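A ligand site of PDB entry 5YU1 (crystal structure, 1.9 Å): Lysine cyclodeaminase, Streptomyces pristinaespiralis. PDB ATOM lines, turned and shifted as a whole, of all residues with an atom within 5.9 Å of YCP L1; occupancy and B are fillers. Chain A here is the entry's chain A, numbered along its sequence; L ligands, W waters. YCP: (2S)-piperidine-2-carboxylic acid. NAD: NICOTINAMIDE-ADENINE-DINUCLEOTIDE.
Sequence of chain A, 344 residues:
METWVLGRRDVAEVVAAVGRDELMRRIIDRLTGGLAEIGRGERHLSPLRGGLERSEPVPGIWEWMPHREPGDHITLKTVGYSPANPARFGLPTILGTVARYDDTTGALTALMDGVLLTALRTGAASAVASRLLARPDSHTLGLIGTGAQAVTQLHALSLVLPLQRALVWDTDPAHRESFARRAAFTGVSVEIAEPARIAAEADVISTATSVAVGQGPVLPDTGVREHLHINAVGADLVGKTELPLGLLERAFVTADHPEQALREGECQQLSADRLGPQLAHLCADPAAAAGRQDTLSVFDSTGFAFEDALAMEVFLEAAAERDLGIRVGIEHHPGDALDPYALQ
An oxygen (O3D) of NAD L2 lies within hydrogen-bond range of the side-chain carboxylate (OD1) of Asp 236 (2.9 Å). O7N of NAD L2 is in hydrogen-bond range of NH1 of Arg 121 (2.7 Å). An oxygen (O) of YCP L1 is in salt-bridge range of the guanidinium group (NH1) of Arg 49 (3.9 Å). The guanidinium group (NH2) of Arg 121 is in salt-bridge range of an oxygen (O) of YCP L1, 2.7 Å away. The backbone carbonyl oxygen (O) of Ala 235 lies within hydrogen-bond range of an oxygen (O2D) of NAD L2 (2.6 Å). N of YCP L1 lies within hydrogen-bond range of O of Thr 302. The side-chain amino group (NZ) of Lys 77 is in salt-bridge range of an oxygen (OXT) of YCP L1, 2.9 Å away. N of Gly 303 lies close to O7N of NAD L2 (3.3 Å). N of Ala 235 lies within hydrogen-bond range of O3D of NAD L2 (3.2 Å).
The side-chain carboxylate (OE1) of Glu 307 lies within salt-bridge range of the guanidinium group (NH1) of Arg 121 (3.6 Å). NH1 of Arg 121 sits at hydrogen-bond distance from OG1 of Thr 122. The side-chain carboxylate of Asp 308 lies within salt-bridge range of the guanidinium group of Arg 121 (2.9 Å). N of Glu 63 sits at hydrogen-bond distance from O of Val 79. O of Gly 303 lies within hydrogen-bond range of NH1 of Arg 49 (2.8 Å). The backbone carbonyl oxygen of Thr 302 sits at hydrogen-bond distance from the guanidinium group of Arg 49, 3.2 Å away. The side-chain carboxylate (OD1) of Asp 308 lies within salt-bridge range of the side-chain amino group (NZ) of Lys 77, 2.6 Å away. NZ of Lys 77 lies within hydrogen-bond range of OG1 of Thr 118, at 2.8 Å.
Merely in contact with YCP L1: Glu 63, Met 65, Ile 94, Thr 118, Ala 235 and Gly 303. Within 4 Å of YCP L1: Arg 49, Glu 63, Met 65, Lys 77, Ile 94, Thr 118, Arg 121, Ala 235, Thr 302 and Gly 303. The nearest printed residue that does not touch YCP L1 is Val 79 (4.02 Å).
Water W1 lies within hydrogen-bond range of the side-chain carboxylate of Glu 63 and the backbone carbonyl oxygen of Val 79.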
ATOM      1  N   ARG A  49     -23.229 -19.952   5.518  1.00  0.00           N
ATOM      2  CA  ARG A  49     -24.275 -20.486   4.660  1.00  0.00           C
ATOM      3  C   ARG A  49     -25.080 -21.559   5.394  1.00  0.00           C
ATOM      4  O   ARG A  49     -24.668 -22.086   6.429  1.00  0.00           O
ATOM      5  CB  ARG A  49     -23.689 -21.070   3.380  1.00  0.00           C
ATOM      6  CG  ARG A  49     -22.755 -22.227   3.608  1.00  0.00           C
ATOM      7  CD  ARG A  49     -22.393 -22.870   2.278  1.00  0.00           C
ATOM      8  NE  ARG A  49     -21.261 -23.792   2.402  1.00  0.00           N
ATOM      9  CZ  ARG A  49     -20.030 -23.523   1.975  1.00  0.00           C
ATOM     10  NH1 ARG A  49     -19.757 -22.367   1.389  1.00  0.00           N
ATOM     11  NH2 ARG A  49     -19.073 -24.431   2.122  1.00  0.00           N
ATOM     12  N   ILE A  61     -25.938 -32.115  -1.286  1.00  0.00           N
ATOM     13  CA  ILE A  61     -26.433 -31.019  -0.456  1.00  0.00           C
ATOM     14  C   ILE A  61     -26.909 -29.900  -1.373  1.00  0.00           C
ATOM     15  O   ILE A  61     -26.483 -29.779  -2.522  1.00  0.00           O
ATOM     16  CB  ILE A  61     -25.348 -30.531   0.550  1.00  0.00           C
ATOM     17  CG1 ILE A  61     -25.978 -29.692   1.669  1.00  0.00           C
ATOM     18  CG2 ILE A  61     -24.199 -29.796  -0.156  1.00  0.00           C
ATOM     19  CD1 ILE A  61     -25.110 -29.584   2.925  1.00  0.00           C
ATOM     20  N   GLU A  63     -27.582 -25.670  -0.908  1.00  0.00           N
ATOM     21  CA  GLU A  63     -27.172 -24.647   0.035  1.00  0.00           C
ATOM     22  C   GLU A  63     -27.603 -23.271  -0.444  1.00  0.00           C
ATOM     23  O   GLU A  63     -27.783 -23.021  -1.646  1.00  0.00           O
ATOM     24  CB  GLU A  63     -25.638 -24.679   0.244  1.00  0.00           C
ATOM     25  CG  GLU A  63     -25.155 -25.963   0.930  1.00  0.00           C
ATOM     26  CD  GLU A  63     -23.630 -26.119   0.937  1.00  0.00           C
ATOM     27  OE1 GLU A  63     -22.971 -25.622   0.003  1.00  0.00           O
ATOM     28  OE2 GLU A  63     -23.103 -26.754   1.886  1.00  0.00           O
ATOM     29  N   MET A  65     -26.621 -19.026   0.265  1.00  0.00           N
ATOM     30  CA  MET A  65     -25.483 -18.211   0.676  1.00  0.00           C
ATOM     31  C   MET A  65     -25.819 -16.743   0.452  1.00  0.00           C
ATOM     32  O   MET A  65     -25.699 -16.240  -0.685  1.00  0.00           O
ATOM     33  CB  MET A  65     -24.226 -18.608  -0.095  1.00  0.00           C
ATOM     34  CG  MET A  65     -23.995 -20.120  -0.180  1.00  0.00           C
ATOM     35  SD  MET A  65     -22.812 -20.613  -1.438  1.00  0.00           S
ATOM     36  CE  MET A  65     -21.356 -19.703  -0.904  1.00  0.00           C
ATOM     37  N   LYS A  77     -26.876 -16.636  -3.424  1.00  0.00           N
ATOM     38  CA  LYS A  77     -26.612 -17.773  -4.295  1.00  0.00           C
ATOM     39  C   LYS A  77     -27.268 -19.018  -3.717  1.00  0.00           C
ATOM     40  O   LYS A  77     -27.136 -19.310  -2.512  1.00  0.00           O
ATOM     41  CB  LYS A  77     -25.117 -18.024  -4.511  1.00  0.00           C
ATOM     42  CG  LYS A  77     -24.900 -19.151  -5.556  1.00  0.00           C
ATOM     43  CD  LYS A  77     -23.487 -19.223  -6.087  1.00  0.00           C
ATOM     44  CE  LYS A  77     -22.629 -20.194  -5.295  1.00  0.00           C
ATOM     45  NZ  LYS A  77     -21.227 -20.151  -5.768  1.00  0.00           N
ATOM     46  N   VAL A  79     -27.285 -23.128  -4.541  1.00  0.00           N
ATOM     47  CA  VAL A  79     -26.407 -24.019  -5.292  1.00  0.00           C
ATOM     48  C   VAL A  79     -26.548 -25.437  -4.762  1.00  0.00           C
ATOM     49  O   VAL A  79     -26.588 -25.672  -3.548  1.00  0.00           O
ATOM     50  CB  VAL A  79     -24.946 -23.528  -5.251  1.00  0.00           C
ATOM     51  CG1 VAL A  79     -24.463 -23.388  -3.815  1.00  0.00           C
ATOM     52  CG2 VAL A  79     -24.034 -24.425  -6.063  1.00  0.00           C
ATOM     53  N   GLY A  80     -26.688 -26.384  -5.691  1.00  0.00           N
ATOM     54  CA  GLY A  80     -26.740 -27.787  -5.367  1.00  0.00           C
ATOM     55  C   GLY A  80     -25.418 -28.458  -5.659  1.00  0.00           C
ATOM     56  O   GLY A  80     -24.690 -28.084  -6.584  1.00  0.00           O
ATOM     57  N   TYR A  81     -25.094 -29.433  -4.820  1.00  0.00           N
ATOM     58  CA  TYR A  81     -23.998 -30.377  -5.028  1.00  0.00           C
ATOM     59  C   TYR A  81     -24.637 -31.739  -5.157  1.00  0.00           C
ATOM     60  O   TYR A  81     -25.264 -32.235  -4.204  1.00  0.00           O
ATOM     61  CB  TYR A  81     -22.994 -30.319  -3.877  1.00  0.00           C
ATOM     62  CG  TYR A  81     -22.060 -31.510  -3.821  1.00  0.00           C
ATOM     63  CD1 TYR A  81     -20.979 -31.613  -4.700  1.00  0.00           C
ATOM     64  CD2 TYR A  81     -22.255 -32.524  -2.885  1.00  0.00           C
ATOM     65  CE1 TYR A  81     -20.105 -32.701  -4.650  1.00  0.00           C
ATOM     66  CE2 TYR A  81     -21.389 -33.619  -2.821  1.00  0.00           C
ATOM     67  CZ  TYR A  81     -20.316 -33.701  -3.702  1.00  0.00           C
ATOM     68  OH  TYR A  81     -19.453 -34.760  -3.625  1.00  0.00           O
ATOM     69  N   ILE A  94     -22.356 -29.317  -9.833  1.00  0.00           N
ATOM     70  CA  ILE A  94     -22.663 -28.044  -9.216  1.00  0.00           C
ATOM     71  C   ILE A  94     -23.653 -27.317 -10.113  1.00  0.00           C
ATOM     72  O   ILE A  94     -23.331 -26.980 -11.266  1.00  0.00           O
ATOM     73  CB  ILE A  94     -21.402 -27.192  -8.980  1.00  0.00           C
ATOM     74  CG1 ILE A  94     -20.432 -27.891  -7.997  1.00  0.00           C
ATOM     75  CG2 ILE A  94     -21.751 -25.784  -8.495  1.00  0.00           C
ATOM     76  CD1 ILE A  94     -20.992 -28.075  -6.562  1.00  0.00           C
ATOM     77  N   THR A 118     -19.747 -19.731 -10.531  1.00  0.00           N
ATOM     78  CA  THR A 118     -19.157 -20.499  -9.423  1.00  0.00           C
ATOM     79  C   THR A 118     -17.778 -21.039  -9.797  1.00  0.00           C
ATOM     80  O   THR A 118     -16.815 -20.908  -9.040  1.00  0.00           O
ATOM     81  CB  THR A 118     -20.089 -21.640  -9.000  1.00  0.00           C
ATOM     82  OG1 THR A 118     -21.287 -21.094  -8.431  1.00  0.00           O
ATOM     83  CG2 THR A 118     -19.400 -22.557  -7.956  1.00  0.00           C
ATOM     84  N   ARG A 121     -15.197 -18.012  -9.995  1.00  0.00           N
ATOM     85  CA  ARG A 121     -14.690 -17.404  -8.766  1.00  0.00           C
ATOM     86  C   ARG A 121     -13.970 -18.406  -7.890  1.00  0.00           C
ATOM     87  O   ARG A 121     -13.134 -17.997  -7.074  1.00  0.00           O
ATOM     88  CB  ARG A 121     -15.811 -16.688  -7.984  1.00  0.00           C
ATOM     89  CG  ARG A 121     -16.985 -17.559  -7.524  1.00  0.00           C
ATOM     90  CD  ARG A 121     -16.663 -18.321  -6.265  1.00  0.00           C
ATOM     91  NE  ARG A 121     -17.820 -18.523  -5.392  1.00  0.00           N
ATOM     92  CZ  ARG A 121     -17.945 -19.556  -4.573  1.00  0.00           C
ATOM     93  NH1 ARG A 121     -16.990 -20.489  -4.530  1.00  0.00           N
ATOM     94  NH2 ARG A 121     -19.010 -19.662  -3.776  1.00  0.00           N
ATOM     95  N   THR A 122     -14.262 -19.696  -8.032  1.00  0.00           N
ATOM     96  CA  THR A 122     -13.548 -20.713  -7.280  1.00  0.00           C
ATOM     97  C   THR A 122     -12.119 -20.853  -7.788  1.00  0.00           C
ATOM     98  O   THR A 122     -11.167 -20.918  -6.994  1.00  0.00           O
ATOM     99  CB  THR A 122     -14.293 -22.047  -7.367  1.00  0.00           C
ATOM    100  OG1 THR A 122     -15.624 -21.856  -6.858  1.00  0.00           O
ATOM    101  CG2 THR A 122     -13.606 -23.133  -6.554  1.00  0.00           C
ATOM    102  N   ALA A 235     -15.460 -29.503  -0.999  1.00  0.00           N
ATOM    103  CA  ALA A 235     -16.255 -29.103   0.155  1.00  0.00           C
ATOM    104  C   ALA A 235     -17.726 -29.291  -0.177  1.00  0.00           C
ATOM    105  O   ALA A 235     -18.181 -28.851  -1.238  1.00  0.00           O
ATOM    106  CB  ALA A 235     -16.004 -27.643   0.554  1.00  0.00           C
ATOM    107  N   ASP A 236     -18.467 -29.940   0.715  1.00  0.00           N
ATOM    108  CA  ASP A 236     -19.913 -30.081   0.540  1.00  0.00           C
ATOM    109  C   ASP A 236     -20.575 -30.475   1.867  1.00  0.00           C
ATOM    110  O   ASP A 236     -21.109 -29.620   2.564  1.00  0.00           O
ATOM    111  CB  ASP A 236     -20.234 -31.090  -0.572  1.00  0.00           C
ATOM    112  CG  ASP A 236     -19.323 -32.331  -0.538  1.00  0.00           C
ATOM    113  OD1 ASP A 236     -18.433 -32.470  -1.401  1.00  0.00           O
ATOM    114  OD2 ASP A 236     -19.521 -33.198   0.352  1.00  0.00           O
ATOM    115  N   GLU A 264     -16.968 -27.151   7.370  1.00  0.00           N
ATOM    116  CA  GLU A 264     -17.060 -27.866   6.112  1.00  0.00           C
ATOM    117  C   GLU A 264     -15.757 -27.990   5.335  1.00  0.00           C
ATOM    118  O   GLU A 264     -15.747 -28.658   4.301  1.00  0.00           O
ATOM    119  CB  GLU A 264     -18.114 -27.196   5.187  1.00  0.00           C
ATOM    120  CG  GLU A 264     -19.553 -27.366   5.684  1.00  0.00           C
ATOM    121  CD  GLU A 264     -20.581 -26.510   4.914  1.00  0.00           C
ATOM    122  OE1 GLU A 264     -20.538 -26.482   3.662  1.00  0.00           O
ATOM    123  OE2 GLU A 264     -21.460 -25.899   5.564  1.00  0.00           O
ATOM    124  N   THR A 302     -13.746 -23.075   0.993  1.00  0.00           N
ATOM    125  CA  THR A 302     -15.121 -23.538   1.051  1.00  0.00           C
ATOM    126  C   THR A 302     -16.051 -22.743   0.161  1.00  0.00           C
ATOM    127  O   THR A 302     -17.131 -23.231  -0.167  1.00  0.00           O
ATOM    128  CB  THR A 302     -15.640 -23.464   2.501  1.00  0.00           C
ATOM    129  OG1 THR A 302     -15.668 -22.086   2.936  1.00  0.00           O
ATOM    130  CG2 THR A 302     -14.734 -24.279   3.411  1.00  0.00           C
ATOM    131  N   GLY A 303     -15.645 -21.541  -0.253  1.00  0.00           N
ATOM    132  CA  GLY A 303     -16.514 -20.622  -0.967  1.00  0.00           C
ATOM    133  C   GLY A 303     -17.379 -19.846  -0.007  1.00  0.00           C
ATOM    134  O   GLY A 303     -17.849 -20.415   0.993  1.00  0.00           O
ATOM    135  N   PHE A 304     -17.560 -18.558  -0.240  1.00  0.00           N
ATOM    136  CA  PHE A 304     -18.523 -17.808   0.557  1.00  0.00           C
ATOM    137  C   PHE A 304     -19.150 -16.741  -0.314  1.00  0.00           C
ATOM    138  O   PHE A 304     -18.638 -16.394  -1.394  1.00  0.00           O
ATOM    139  CB  PHE A 304     -17.908 -17.230   1.866  1.00  0.00           C
ATOM    140  CG  PHE A 304     -16.792 -16.229   1.672  1.00  0.00           C
ATOM    141  CD1 PHE A 304     -15.504 -16.643   1.305  1.00  0.00           C
ATOM    142  CD2 PHE A 304     -16.998 -14.893   1.946  1.00  0.00           C
ATOM    143  CE1 PHE A 304     -14.483 -15.731   1.145  1.00  0.00           C
ATOM    144  CE2 PHE A 304     -15.962 -13.963   1.803  1.00  0.00           C
ATOM    145  CZ  PHE A 304     -14.702 -14.388   1.401  1.00  0.00           C
ATOM    146  N   GLU A 307     -17.751 -13.744  -2.459  1.00  0.00           N
ATOM    147  CA  GLU A 307     -17.087 -14.055  -3.724  1.00  0.00           C
ATOM    148  C   GLU A 307     -18.086 -14.096  -4.873  1.00  0.00           C
ATOM    149  O   GLU A 307     -17.790 -13.605  -5.960  1.00  0.00           O
ATOM    150  CB  GLU A 307     -16.351 -15.397  -3.630  1.00  0.00           C
ATOM    151  CG  GLU A 307     -15.354 -15.488  -2.483  1.00  0.00           C
ATOM    152  CD  GLU A 307     -14.667 -16.843  -2.380  1.00  0.00           C
ATOM    153  OE1 GLU A 307     -15.329 -17.865  -2.634  1.00  0.00           O
ATOM    154  OE2 GLU A 307     -13.472 -16.885  -2.039  1.00  0.00           O
ATOM    155  N   ASP A 308     -19.261 -14.689  -4.637  1.00  0.00           N
ATOM    156  CA  ASP A 308     -20.314 -14.699  -5.660  1.00  0.00           C
ATOM    157  C   ASP A 308     -20.854 -13.313  -5.942  1.00  0.00           C
ATOM    158  O   ASP A 308     -21.167 -12.992  -7.100  1.00  0.00           O
ATOM    159  CB  ASP A 308     -21.444 -15.627  -5.214  1.00  0.00           C
ATOM    160  CG  ASP A 308     -20.960 -17.035  -4.968  1.00  0.00           C
ATOM    161  OD1 ASP A 308     -20.499 -17.652  -5.941  1.00  0.00           O
ATOM    162  OD2 ASP A 308     -21.036 -17.513  -3.801  1.00  0.00           O
HETATM  163  C   YCP L   1     -19.862 -22.899  -3.271  1.00  0.00           C
HETATM  164  N   YCP L   1     -19.421 -24.556  -1.597  1.00  0.00           N
HETATM  165  O   YCP L   1     -19.358 -22.040  -2.480  1.00  0.00           O
HETATM  166  CA  YCP L   1     -19.616 -24.356  -3.037  1.00  0.00           C
HETATM  167  CB  YCP L   1     -20.788 -25.167  -3.568  1.00  0.00           C
HETATM  168  CD  YCP L   1     -20.501 -26.754  -1.733  1.00  0.00           C
HETATM  169  CE  YCP L   1     -19.304 -25.981  -1.233  1.00  0.00           C
HETATM  170  CG  YCP L   1     -20.679 -26.571  -3.170  1.00  0.00           C
HETATM  171  OXT YCP L   1     -20.559 -22.551  -4.258  1.00  0.00           O
HETATM  172  PA  NAD L   2     -17.368 -32.882 -10.465  1.00  0.00           P
HETATM  173  O1A NAD L   2     -18.332 -33.997 -10.150  1.00  0.00           O
HETATM  174  O2A NAD L   2     -17.414 -32.113 -11.772  1.00  0.00           O
HETATM  175  O5B NAD L   2     -15.853 -33.373 -10.271  1.00  0.00           O
HETATM  176  C5B NAD L   2     -15.506 -34.147  -9.131  1.00  0.00           C
HETATM  177  C4B NAD L   2     -14.529 -35.209  -9.618  1.00  0.00           C
HETATM  178  O4B NAD L   2     -13.893 -35.817  -8.492  1.00  0.00           O
HETATM  179  C3B NAD L   2     -15.201 -36.330 -10.414  1.00  0.00           C
HETATM  180  O3B NAD L   2     -14.540 -36.465 -11.684  1.00  0.00           O
HETATM  181  C2B NAD L   2     -14.981 -37.564  -9.556  1.00  0.00           C
HETATM  182  O2B NAD L   2     -14.773 -38.775 -10.284  1.00  0.00           O
HETATM  183  C1B NAD L   2     -13.715 -37.191  -8.822  1.00  0.00           C
HETATM  184  N9A NAD L   2     -13.446 -37.958  -7.596  1.00  0.00           N
HETATM  185  C8A NAD L   2     -14.325 -38.467  -6.705  1.00  0.00           C
HETATM  186  N7A NAD L   2     -13.655 -39.081  -5.677  1.00  0.00           N
HETATM  187  C5A NAD L   2     -12.329 -38.973  -5.932  1.00  0.00           C
HETATM  188  C6A NAD L   2     -11.064 -39.387  -5.302  1.00  0.00           C
HETATM  189  N6A NAD L   2     -11.057 -40.085  -4.145  1.00  0.00           N
HETATM  190  N1A NAD L   2      -9.912 -39.054  -5.921  1.00  0.00           N
HETATM  191  C2A NAD L   2      -9.872 -38.370  -7.070  1.00  0.00           C
HETATM  192  N3A NAD L   2     -10.971 -37.967  -7.714  1.00  0.00           N
HETATM  193  C4A NAD L   2     -12.206 -38.226  -7.198  1.00  0.00           C
HETATM  194  O3  NAD L   2     -17.513 -31.798  -9.267  1.00  0.00           O
HETATM  195  PN  NAD L   2     -16.849 -30.338  -9.231  1.00  0.00           P
HETATM  196  O1N NAD L   2     -15.477 -30.357  -9.828  1.00  0.00           O
HETATM  197  O2N NAD L   2     -17.893 -29.316  -9.639  1.00  0.00           O
HETATM  198  O5D NAD L   2     -16.737 -30.118  -7.630  1.00  0.00           O
HETATM  199  C5D NAD L   2     -15.745 -30.824  -6.866  1.00  0.00           C
HETATM  200  C4D NAD L   2     -15.775 -30.375  -5.408  1.00  0.00           C
HETATM  201  O4D NAD L   2     -15.557 -28.977  -5.327  1.00  0.00           O
HETATM  202  C3D NAD L   2     -17.113 -30.638  -4.719  1.00  0.00           C
HETATM  203  O3D NAD L   2     -16.888 -31.059  -3.349  1.00  0.00           O
HETATM  204  C2D NAD L   2     -17.762 -29.271  -4.737  1.00  0.00           C
HETATM  205  O2D NAD L   2     -18.789 -29.108  -3.751  1.00  0.00           O
HETATM  206  C1D NAD L   2     -16.558 -28.378  -4.504  1.00  0.00           C
HETATM  207  N1N NAD L   2     -16.733 -26.969  -4.823  1.00  0.00           N
HETATM  208  C2N NAD L   2     -16.121 -26.084  -4.036  1.00  0.00           C
HETATM  209  C3N NAD L   2     -16.213 -24.723  -4.269  1.00  0.00           C
HETATM  210  C7N NAD L   2     -15.498 -23.769  -3.369  1.00  0.00           C
HETATM  211  O7N NAD L   2     -15.789 -22.583  -3.417  1.00  0.00           O
HETATM  212  N7N NAD L   2     -14.533 -24.236  -2.546  1.00  0.00           N
HETATM  213  C4N NAD L   2     -16.965 -24.260  -5.354  1.00  0.00           C
HETATM  214  C5N NAD L   2     -17.575 -25.207  -6.174  1.00  0.00           C
HETATM  215  C6N NAD L   2     -17.443 -26.561  -5.900  1.00  0.00           C
HETATM  216  O   HOH W   1     -23.887 -26.982  -2.510  1.00  0.00           O
